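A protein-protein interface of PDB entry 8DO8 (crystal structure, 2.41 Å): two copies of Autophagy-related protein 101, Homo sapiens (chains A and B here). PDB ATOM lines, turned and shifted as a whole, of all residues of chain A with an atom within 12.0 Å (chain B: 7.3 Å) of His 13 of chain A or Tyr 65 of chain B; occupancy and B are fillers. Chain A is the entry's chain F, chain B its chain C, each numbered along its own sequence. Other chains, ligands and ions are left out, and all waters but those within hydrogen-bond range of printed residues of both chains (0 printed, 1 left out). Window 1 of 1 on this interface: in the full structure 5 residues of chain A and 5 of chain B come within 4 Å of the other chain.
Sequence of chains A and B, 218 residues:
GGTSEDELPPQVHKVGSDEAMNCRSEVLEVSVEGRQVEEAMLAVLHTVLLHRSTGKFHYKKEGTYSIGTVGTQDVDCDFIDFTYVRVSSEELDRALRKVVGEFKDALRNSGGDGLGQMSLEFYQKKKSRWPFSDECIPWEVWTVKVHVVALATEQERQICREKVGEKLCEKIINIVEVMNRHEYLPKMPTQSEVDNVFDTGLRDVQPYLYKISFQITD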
ATOM      1  N   LEU A   8      -4.574 -32.992 -11.118  1.00  0.00           N
ATOM      2  CA  LEU A   8      -5.490 -32.048 -10.482  1.00  0.00           C
ATOM      3  C   LEU A   8      -6.396 -31.382 -11.515  1.00  0.00           C
ATOM      4  O   LEU A   8      -5.953 -31.059 -12.617  1.00  0.00           O
ATOM      5  CB  LEU A   8      -4.714 -30.987  -9.695  1.00  0.00           C
ATOM      6  CG  LEU A   8      -4.410 -31.317  -8.229  1.00  0.00           C
ATOM      7  CD1 LEU A   8      -3.270 -30.457  -7.703  1.00  0.00           C
ATOM      8  CD2 LEU A   8      -5.644 -31.162  -7.350  1.00  0.00           C
ATOM      9  N   PRO A   9      -7.659 -31.171 -11.152  1.00  0.00           N
ATOM     10  CA  PRO A   9      -8.627 -30.601 -12.097  1.00  0.00           C
ATOM     11  C   PRO A   9      -8.295 -29.155 -12.406  1.00  0.00           C
ATOM     12  O   PRO A   9      -7.412 -28.564 -11.766  1.00  0.00           O
ATOM     13  CB  PRO A   9      -9.965 -30.707 -11.344  1.00  0.00           C
ATOM     14  CG  PRO A   9      -9.702 -31.553 -10.145  1.00  0.00           C
ATOM     15  CD  PRO A   9      -8.257 -31.395  -9.827  1.00  0.00           C
ATOM     16  N   PRO A  10      -8.968 -28.552 -13.386  1.00  0.00           N
ATOM     17  CA  PRO A  10      -8.839 -27.102 -13.574  1.00  0.00           C
ATOM     18  C   PRO A  10      -9.256 -26.371 -12.308  1.00  0.00           C
ATOM     19  O   PRO A  10     -10.314 -26.640 -11.732  1.00  0.00           O
ATOM     20  CB  PRO A  10      -9.788 -26.805 -14.741  1.00  0.00           C
ATOM     21  CG  PRO A  10      -9.965 -28.112 -15.447  1.00  0.00           C
ATOM     22  CD  PRO A  10      -9.789 -29.189 -14.430  1.00  0.00           C
ATOM     23  N   GLN A  11      -8.404 -25.451 -11.860  1.00  0.00           N
ATOM     24  CA  GLN A  11      -8.669 -24.764 -10.604  1.00  0.00           C
ATOM     25  C   GLN A  11      -9.617 -23.586 -10.781  1.00  0.00           C
ATOM     26  O   GLN A  11     -10.396 -23.284  -9.871  1.00  0.00           O
ATOM     27  CB  GLN A  11      -7.355 -24.302  -9.977  1.00  0.00           C
ATOM     28  CG  GLN A  11      -6.458 -25.443  -9.525  1.00  0.00           C
ATOM     29  CD  GLN A  11      -7.214 -26.528  -8.768  1.00  0.00           C
ATOM     30  OE1 GLN A  11      -7.477 -26.392  -7.573  1.00  0.00           O
ATOM     31  NE2 GLN A  11      -7.560 -27.611  -9.459  1.00  0.00           N
ATOM     32  N   VAL A  12      -9.582 -22.921 -11.936  1.00  0.00           N
ATOM     33  CA  VAL A  12     -10.412 -21.755 -12.196  1.00  0.00           C
ATOM     34  C   VAL A  12     -10.991 -21.877 -13.596  1.00  0.00           C
ATOM     35  O   VAL A  12     -10.471 -22.599 -14.450  1.00  0.00           O
ATOM     36  CB  VAL A  12      -9.630 -20.427 -12.051  1.00  0.00           C
ATOM     37  N   HIS A  13     -12.090 -21.165 -13.820  1.00  0.00           N
ATOM     38  CA  HIS A  13     -12.747 -21.115 -15.120  1.00  0.00           C
ATOM     39  C   HIS A  13     -12.824 -19.661 -15.565  1.00  0.00           C
ATOM     40  O   HIS A  13     -13.272 -18.801 -14.800  1.00  0.00           O
ATOM     41  CB  HIS A  13     -14.147 -21.749 -15.061  1.00  0.00           C
ATOM     42  CG  HIS A  13     -14.143 -23.207 -14.703  1.00  0.00           C
ATOM     43  ND1 HIS A  13     -14.735 -24.170 -15.493  1.00  0.00           N
ATOM     44  CD2 HIS A  13     -13.617 -23.865 -13.641  1.00  0.00           C
ATOM     45  CE1 HIS A  13     -14.574 -25.357 -14.934  1.00  0.00           C
ATOM     46  NE2 HIS A  13     -13.899 -25.200 -13.809  1.00  0.00           N
ATOM     47  N   LYS A  14     -12.379 -19.389 -16.790  1.00  0.00           N
ATOM     48  CA  LYS A  14     -12.354 -18.035 -17.328  1.00  0.00           C
ATOM     49  C   LYS A  14     -13.475 -17.854 -18.344  1.00  0.00           C
ATOM     50  O   LYS A  14     -13.714 -18.727 -19.185  1.00  0.00           O
ATOM     51  CB  LYS A  14     -11.003 -17.718 -17.975  1.00  0.00           C
ATOM     52  N   VAL A  15     -14.158 -16.715 -18.257  1.00  0.00           N
ATOM     53  CA  VAL A  15     -15.254 -16.388 -19.159  1.00  0.00           C
ATOM     54  C   VAL A  15     -14.909 -15.141 -19.956  1.00  0.00           C
ATOM     55  O   VAL A  15     -14.637 -14.090 -19.380  1.00  0.00           O
ATOM     56  CB  VAL A  15     -16.573 -16.188 -18.392  1.00  0.00           C
ATOM     57  N   THR B  54     -25.050 -26.682 -10.940  1.00  0.00           N
ATOM     58  CA  THR B  54     -23.603 -26.778 -10.864  1.00  0.00           C
ATOM     59  C   THR B  54     -23.166 -26.387  -9.462  1.00  0.00           C
ATOM     60  O   THR B  54     -23.985 -26.042  -8.608  1.00  0.00           O
ATOM     61  CB  THR B  54     -22.921 -25.892 -11.912  1.00  0.00           C
ATOM     62  OG1 THR B  54     -21.508 -26.135 -11.885  1.00  0.00           O
ATOM     63  CG2 THR B  54     -23.191 -24.408 -11.625  1.00  0.00           C
ATOM     64  N   GLY B  55     -21.861 -26.446  -9.225  1.00  0.00           N
ATOM     65  CA  GLY B  55     -21.327 -25.921  -7.993  1.00  0.00           C
ATOM     66  C   GLY B  55     -21.485 -24.417  -7.901  1.00  0.00           C
ATOM     67  O   GLY B  55     -21.600 -23.701  -8.897  1.00  0.00           O
ATOM     68  N   LYS B  56     -21.496 -23.932  -6.666  1.00  0.00           N
ATOM     69  CA  LYS B  56     -21.655 -22.507  -6.425  1.00  0.00           C
ATOM     70  C   LYS B  56     -20.444 -21.754  -6.960  1.00  0.00           C
ATOM     71  O   LYS B  56     -19.301 -22.113  -6.669  1.00  0.00           O
ATOM     72  CB  LYS B  56     -21.843 -22.255  -4.933  1.00  0.00           C
ATOM     73  CG  LYS B  56     -23.291 -22.390  -4.498  1.00  0.00           C
ATOM     74  CD  LYS B  56     -23.683 -21.284  -3.530  1.00  0.00           C
ATOM     75  CE  LYS B  56     -24.448 -20.186  -4.242  1.00  0.00           C
ATOM     76  NZ  LYS B  56     -25.357 -19.482  -3.311  1.00  0.00           N
ATOM     77  N   PHE B  57     -20.697 -20.723  -7.762  1.00  0.00           N
ATOM     78  CA  PHE B  57     -19.620 -19.925  -8.338  1.00  0.00           C
ATOM     79  C   PHE B  57     -19.080 -18.934  -7.315  1.00  0.00           C
ATOM     80  O   PHE B  57     -19.840 -18.314  -6.566  1.00  0.00           O
ATOM     81  CB  PHE B  57     -20.101 -19.164  -9.576  1.00  0.00           C
ATOM     82  CG  PHE B  57     -20.309 -20.031 -10.785  1.00  0.00           C
ATOM     83  CD1 PHE B  57     -20.004 -21.380 -10.752  1.00  0.00           C
ATOM     84  CD2 PHE B  57     -20.827 -19.496 -11.951  1.00  0.00           C
ATOM     85  CE1 PHE B  57     -20.208 -22.180 -11.866  1.00  0.00           C
ATOM     86  CE2 PHE B  57     -21.031 -20.289 -13.066  1.00  0.00           C
ATOM     87  CZ  PHE B  57     -20.724 -21.632 -13.023  1.00  0.00           C
ATOM     88  N   HIS B  58     -17.759 -18.795  -7.286  1.00  0.00           N
ATOM     89  CA  HIS B  58     -17.077 -17.826  -6.433  1.00  0.00           C
ATOM     90  C   HIS B  58     -16.126 -17.036  -7.322  1.00  0.00           C
ATOM     91  O   HIS B  58     -15.077 -17.550  -7.726  1.00  0.00           O
ATOM     92  CB  HIS B  58     -16.333 -18.521  -5.288  1.00  0.00           C
ATOM     93  CG  HIS B  58     -17.206 -19.408  -4.456  1.00  0.00           C
ATOM     94  ND1 HIS B  58     -17.849 -18.966  -3.319  1.00  0.00           N
ATOM     95  CD2 HIS B  58     -17.553 -20.711  -4.600  1.00  0.00           C
ATOM     96  CE1 HIS B  58     -18.551 -19.957  -2.798  1.00  0.00           C
ATOM     97  NE2 HIS B  58     -18.389 -21.027  -3.555  1.00  0.00           N
ATOM     98  N   TYR B  59     -16.495 -15.797  -7.640  1.00  0.00           N
ATOM     99  CA  TYR B  59     -15.772 -15.036  -8.650  1.00  0.00           C
ATOM    100  C   TYR B  59     -14.521 -14.394  -8.063  1.00  0.00           C
ATOM    101  O   TYR B  59     -14.537 -13.868  -6.947  1.00  0.00           O
ATOM    102  CB  TYR B  59     -16.681 -13.971  -9.264  1.00  0.00           C
ATOM    103  CG  TYR B  59     -17.613 -14.513 -10.324  1.00  0.00           C
ATOM    104  CD1 TYR B  59     -18.856 -15.029  -9.983  1.00  0.00           C
ATOM    105  CD2 TYR B  59     -17.249 -14.515 -11.666  1.00  0.00           C
ATOM    106  CE1 TYR B  59     -19.716 -15.533 -10.948  1.00  0.00           C
ATOM    107  CE2 TYR B  59     -18.103 -15.019 -12.641  1.00  0.00           C
ATOM    108  CZ  TYR B  59     -19.337 -15.524 -12.273  1.00  0.00           C
ATOM    109  OH  TYR B  59     -20.195 -16.028 -13.228  1.00  0.00           O
ATOM    110  N   LYS B  60     -13.427 -14.457  -8.823  1.00  0.00           N
ATOM    111  CA  LYS B  60     -12.165 -13.814  -8.471  1.00  0.00           C
ATOM    112  C   LYS B  60     -11.937 -12.529  -9.259  1.00  0.00           C
ATOM    113  O   LYS B  60     -11.625 -11.488  -8.675  1.00  0.00           O
ATOM    114  CB  LYS B  60     -10.999 -14.788  -8.692  1.00  0.00           C
ATOM    115  N   LYS B  61     -12.073 -12.585 -10.580  1.00  0.00           N
ATOM    116  CA  LYS B  61     -12.123 -11.409 -11.432  1.00  0.00           C
ATOM    117  C   LYS B  61     -13.526 -11.309 -12.030  1.00  0.00           C
ATOM    118  O   LYS B  61     -14.457 -12.000 -11.599  1.00  0.00           O
ATOM    119  CB  LYS B  61     -11.031 -11.475 -12.505  1.00  0.00           C
ATOM    120  N   GLU B  62     -13.685 -10.447 -13.032  1.00  0.00           N
ATOM    121  CA  GLU B  62     -14.997 -10.283 -13.647  1.00  0.00           C
ATOM    122  C   GLU B  62     -15.421 -11.550 -14.377  1.00  0.00           C
ATOM    123  O   GLU B  62     -16.560 -12.014 -14.229  1.00  0.00           O
ATOM    124  CB  GLU B  62     -14.987  -9.088 -14.602  1.00  0.00           C
ATOM    125  CG  GLU B  62     -16.171  -9.047 -15.553  1.00  0.00           C
ATOM    126  CD  GLU B  62     -17.464  -8.645 -14.866  1.00  0.00           C
ATOM    127  OE1 GLU B  62     -17.427  -8.329 -13.656  1.00  0.00           O
ATOM    128  OE2 GLU B  62     -18.520  -8.647 -15.537  1.00  0.00           O
ATOM    129  N   GLY B  63     -14.519 -12.124 -15.166  1.00  0.00           N
ATOM    130  CA  GLY B  63     -14.821 -13.325 -15.915  1.00  0.00           C
ATOM    131  C   GLY B  63     -14.031 -14.532 -15.456  1.00  0.00           C
ATOM    132  O   GLY B  63     -13.920 -15.519 -16.187  1.00  0.00           O
ATOM    133  N   THR B  64     -13.474 -14.463 -14.250  1.00  0.00           N
ATOM    134  CA  THR B  64     -12.726 -15.563 -13.657  1.00  0.00           C
ATOM    135  C   THR B  64     -13.421 -15.997 -12.374  1.00  0.00           C
ATOM    136  O   THR B  64     -13.743 -15.161 -11.525  1.00  0.00           O
ATOM    137  CB  THR B  64     -11.275 -15.154 -13.371  1.00  0.00           C
ATOM    138  OG1 THR B  64     -10.500 -15.259 -14.571  1.00  0.00           O
ATOM    139  CG2 THR B  64     -10.661 -16.041 -12.302  1.00  0.00           C
ATOM    140  N   TYR B  65     -13.662 -17.298 -12.240  1.00  0.00           N
ATOM    141  CA  TYR B  65     -14.321 -17.828 -11.057  1.00  0.00           C
ATOM    142  C   TYR B  65     -13.911 -19.282 -10.863  1.00  0.00           C
ATOM    143  O   TYR B  65     -13.293 -19.904 -11.734  1.00  0.00           O
ATOM    144  CB  TYR B  65     -15.849 -17.718 -11.158  1.00  0.00           C
ATOM    145  CG  TYR B  65     -16.437 -18.502 -12.311  1.00  0.00           C
ATOM    146  CD1 TYR B  65     -16.486 -17.964 -13.593  1.00  0.00           C
ATOM    147  CD2 TYR B  65     -16.914 -19.792 -12.121  1.00  0.00           C
ATOM    148  CE1 TYR B  65     -17.018 -18.681 -14.650  1.00  0.00           C
ATOM    149  CE2 TYR B  65     -17.441 -20.522 -13.171  1.00  0.00           C
ATOM    150  CZ  TYR B  65     -17.491 -19.964 -14.432  1.00  0.00           C
ATOM    151  OH  TYR B  65     -18.016 -20.692 -15.473  1.00  0.00           O
ATOM    152  N   SER B  66     -14.273 -19.821  -9.703  1.00  0.00           N
ATOM    153  CA  SER B  66     -14.055 -21.222  -9.384  1.00  0.00           C
ATOM    154  C   SER B  66     -15.373 -21.821  -8.919  1.00  0.00           C
ATOM    155  O   SER B  66     -16.314 -21.105  -8.568  1.00  0.00           O
ATOM    156  CB  SER B  66     -12.975 -21.396  -8.313  1.00  0.00           C
ATOM    157  OG  SER B  66     -13.268 -20.595  -7.187  1.00  0.00           O
ATOM    158  N   ILE B  67     -15.438 -23.149  -8.920  1.00  0.00           N
ATOM    159  CA  ILE B  67     -16.692 -23.865  -8.744  1.00  0.00           C
ATOM    160  C   ILE B  67     -16.595 -24.770  -7.523  1.00  0.00           C
ATOM    161  O   ILE B  67     -15.578 -25.440  -7.309  1.00  0.00           O
ATOM    162  CB  ILE B  67     -17.049 -24.674 -10.012  1.00  0.00           C
ATOM    163  CG1 ILE B  67     -17.002 -23.776 -11.250  1.00  0.00           C
ATOM    164  CG2 ILE B  67     -18.433 -25.278  -9.897  1.00  0.00           C
ATOM    165  CD1 ILE B  67     -16.936 -24.537 -12.550  1.00  0.00           C
ATOM    166  N   MET B 188     -21.867 -19.154 -20.244  1.00  0.00           N
ATOM    167  CA  MET B 188     -21.428 -19.059 -18.854  1.00  0.00           C
ATOM    168  C   MET B 188     -21.134 -17.602 -18.508  1.00  0.00           C
ATOM    169  O   MET B 188     -20.433 -16.914 -19.263  1.00  0.00           O
ATOM    170  CB  MET B 188     -20.206 -19.933 -18.593  1.00  0.00           C
ATOM    171  CG  MET B 188     -20.549 -21.433 -18.531  1.00  0.00           C
ATOM    172  SD  MET B 188     -21.605 -21.888 -17.126  1.00  0.00           S
ATOM    173  CE  MET B 188     -21.713 -23.673 -17.312  1.00  0.00           C
ATOM    174  N   PRO B 189     -21.646 -17.097 -17.392  1.00  0.00           N
ATOM    175  CA  PRO B 189     -21.691 -15.652 -17.176  1.00  0.00           C
ATOM    176  C   PRO B 189     -20.454 -15.098 -16.486  1.00  0.00           C
ATOM    177  O   PRO B 189     -19.721 -15.800 -15.787  1.00  0.00           O
ATOM    178  CB  PRO B 189     -22.923 -15.491 -16.276  1.00  0.00           C
ATOM    179  CG  PRO B 189     -22.939 -16.751 -15.463  1.00  0.00           C
ATOM    180  CD  PRO B 189     -22.300 -17.842 -16.301  1.00  0.00           C
ATOM    181  N   THR B 190     -20.238 -13.803 -16.710  1.00  0.00           N
ATOM    182  CA  THR B 190     -19.342 -13.030 -15.869  1.00  0.00           C
ATOM    183  C   THR B 190     -20.023 -12.743 -14.531  1.00  0.00           C
ATOM    184  O   THR B 190     -21.211 -13.022 -14.340  1.00  0.00           O
ATOM    185  CB  THR B 190     -18.945 -11.725 -16.563  1.00  0.00           C
ATOM    186  N   GLN B 191     -19.258 -12.168 -13.597  1.00  0.00           N
ATOM    187  CA  GLN B 191     -19.812 -11.893 -12.273  1.00  0.00           C
ATOM    188  C   GLN B 191     -21.026 -10.973 -12.348  1.00  0.00           C
ATOM    189  O   GLN B 191     -21.922 -11.057 -11.500  1.00  0.00           O
ATOM    190  CB  GLN B 191     -18.744 -11.288 -11.363  1.00  0.00           C
ATOM    191  CG  GLN B 191     -19.273 -10.879  -9.989  1.00  0.00           C
ATOM    192  CD  GLN B 191     -18.182 -10.766  -8.946  1.00  0.00           C
ATOM    193  OE1 GLN B 191     -17.043 -10.420  -9.256  1.00  0.00           O
ATOM    194  NE2 GLN B 191     -18.524 -11.067  -7.697  1.00  0.00           N
ATOM    195  N   VAL B 194     -24.190 -13.252 -13.514  1.00  0.00           N
ATOM    196  CA  VAL B 194     -24.382 -14.557 -12.889  1.00  0.00           C
ATOM    197  C   VAL B 194     -25.787 -14.723 -12.323  1.00  0.00           C
ATOM    198  O   VAL B 194     -26.286 -15.850 -12.211  1.00  0.00           O
ATOM    199  CB  VAL B 194     -23.298 -14.780 -11.816  1.00  0.00           C
ATOM    200  CG1 VAL B 194     -23.610 -13.981 -10.559  1.00  0.00           C
ATOM    201  CG2 VAL B 194     -23.163 -16.261 -11.501  1.00  0.00           C
ATOM    202  N   PHE B 198     -28.211 -18.029 -13.157  1.00  0.00           N
ATOM    203  CA  PHE B 198     -28.228 -19.022 -12.097  1.00  0.00           C
ATOM    204  C   PHE B 198     -28.991 -18.511 -10.885  1.00  0.00           C
ATOM    205  O   PHE B 198     -29.069 -17.304 -10.637  1.00  0.00           O
ATOM    206  CB  PHE B 198     -26.807 -19.398 -11.680  1.00  0.00           C
ATOM    207  CG  PHE B 198     -26.110 -20.293 -12.654  1.00  0.00           C
ATOM    208  CD1 PHE B 198     -26.463 -21.633 -12.763  1.00  0.00           C
ATOM    209  CD2 PHE B 198     -25.098 -19.800 -13.462  1.00  0.00           C
ATOM    210  CE1 PHE B 198     -25.812 -22.465 -13.653  1.00  0.00           C
ATOM    211  CE2 PHE B 198     -24.444 -20.629 -14.359  1.00  0.00           C
ATOM    212  CZ  PHE B 198     -24.801 -21.963 -14.455  1.00  0.00           C
ATOM    213  N   GLN B 206     -26.051 -24.735  -7.044  1.00  0.00           N
ATOM    214  CA  GLN B 206     -26.329 -23.579  -7.899  1.00  0.00           C
ATOM    215  C   GLN B 206     -27.136 -24.005  -9.120  1.00  0.00           C
ATOM    216  O   GLN B 206     -26.564 -24.354 -10.166  1.00  0.00           O
ATOM    217  CB  GLN B 206     -25.032 -22.899  -8.323  1.00  0.00           C
ATOM    218  CG  GLN B 206     -25.235 -21.647  -9.148  1.00  0.00           C
ATOM    219  CD  GLN B 206     -23.927 -21.001  -9.543  1.00  0.00           C
ATOM    220  OE1 GLN B 206     -23.238 -20.420  -8.707  1.00  0.00           O
ATOM    221  NE2 GLN B 206     -23.569 -21.110 -10.820  1.00  0.00           N
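The backbone carbonyl oxygen (O) of Gly 63 of chain B sits at hydrogen-bond distance from the backbone NH (N) of Val 15 of chain A (2.4 Å). O of Tyr 65 of chain B is in hydrogen-bond range of N of His 13 of chain A, at 2.7 Å.
N of His 58 of chain B sits at hydrogen-bond distance from O of Ser 66 of chain B, 3.0 Å away. The backbone carbonyl oxygen (O) of Pro 9 of chain A sits at hydrogen-bond distance from the side-chain amide nitrogen (NE2) of Gln 11 of chain A, at 2.5 Å.
Among the printed residues, merely in contact across the chains: Lys 14 of chain A with Gly 63 of chain B, His 13 of chain A with Ile 67 of chain B, Val 12 of chain A with Tyr 65 of chain B, His 13 of chain A with Thr 64 of chain B, Gln 11 of chain A with Ser 66 of chain B and His 13 of chain A with Gly 63 of chain B.
His 13 of chain A touches just these residues of chain B: Gly 63, Thr 64, Tyr 65 and Ile 67. Of chain A, only Val 12 and His 13 come within 4 Å of Tyr 65 of chain B. No residue of chain A comes within 4 Å of Phe 57 of chain B. No residue of chain A comes within 4 Å of Lys 60 of chain B. No residue of chain A comes within 4 Å of Lys 61 of chain B. Of chain A, only His 13 (3.6 Å), Lys 14 (3.2 Å) and Val 15 (2.4 Å) come within 4 Å of Gly 63 of chain B. Ser 66 of chain B touches just one residue of chain A: Gln 11. Of chain A, only His 13 (3.4 Å) comes within 4 Å of Ile 67 of chain B. No residue of chain A comes within 4 Å of Met 188 of chain B. No residue of chain A comes within 4 Å of Thr 190 of chain B. Of the printed residues of chain B, Val 15 of chain A touches Gly 63 (2.4 Å). Of the printed residues of chain B, Val 12 of chain A touches Tyr 65 (3.5 Å). Printed residues of chain B within 4 Å of Lys 14 of chain A: Gly 63. Of the printed residues of chain B, Gln 11 of chain A touches Ser 66 (3.6 Å). The nearest residue of chain B that does not touch His 13 of chain A is Ser 66 of chain B (4.8 Å). The nearest printed residue of chain B that does not touch Val 15 of chain A is Met 188 of chain B (4.02 Å).
Printed residues of chain A that touch a printed residue of chain B: Gln 11, Val 12, His 13, Lys 14 and Val 15. Among the printed residues, 8 pairs touch across the chains. Among the printed residues, no Asp or Glu carboxylate lies within 4 Å of a Lys or Arg side-chain nitrogen of the other chain.
No position is printed for both chains. Of the 8 pairs that touch across the chains among the printed residues, none has its exchanged pair printed and touching as well.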
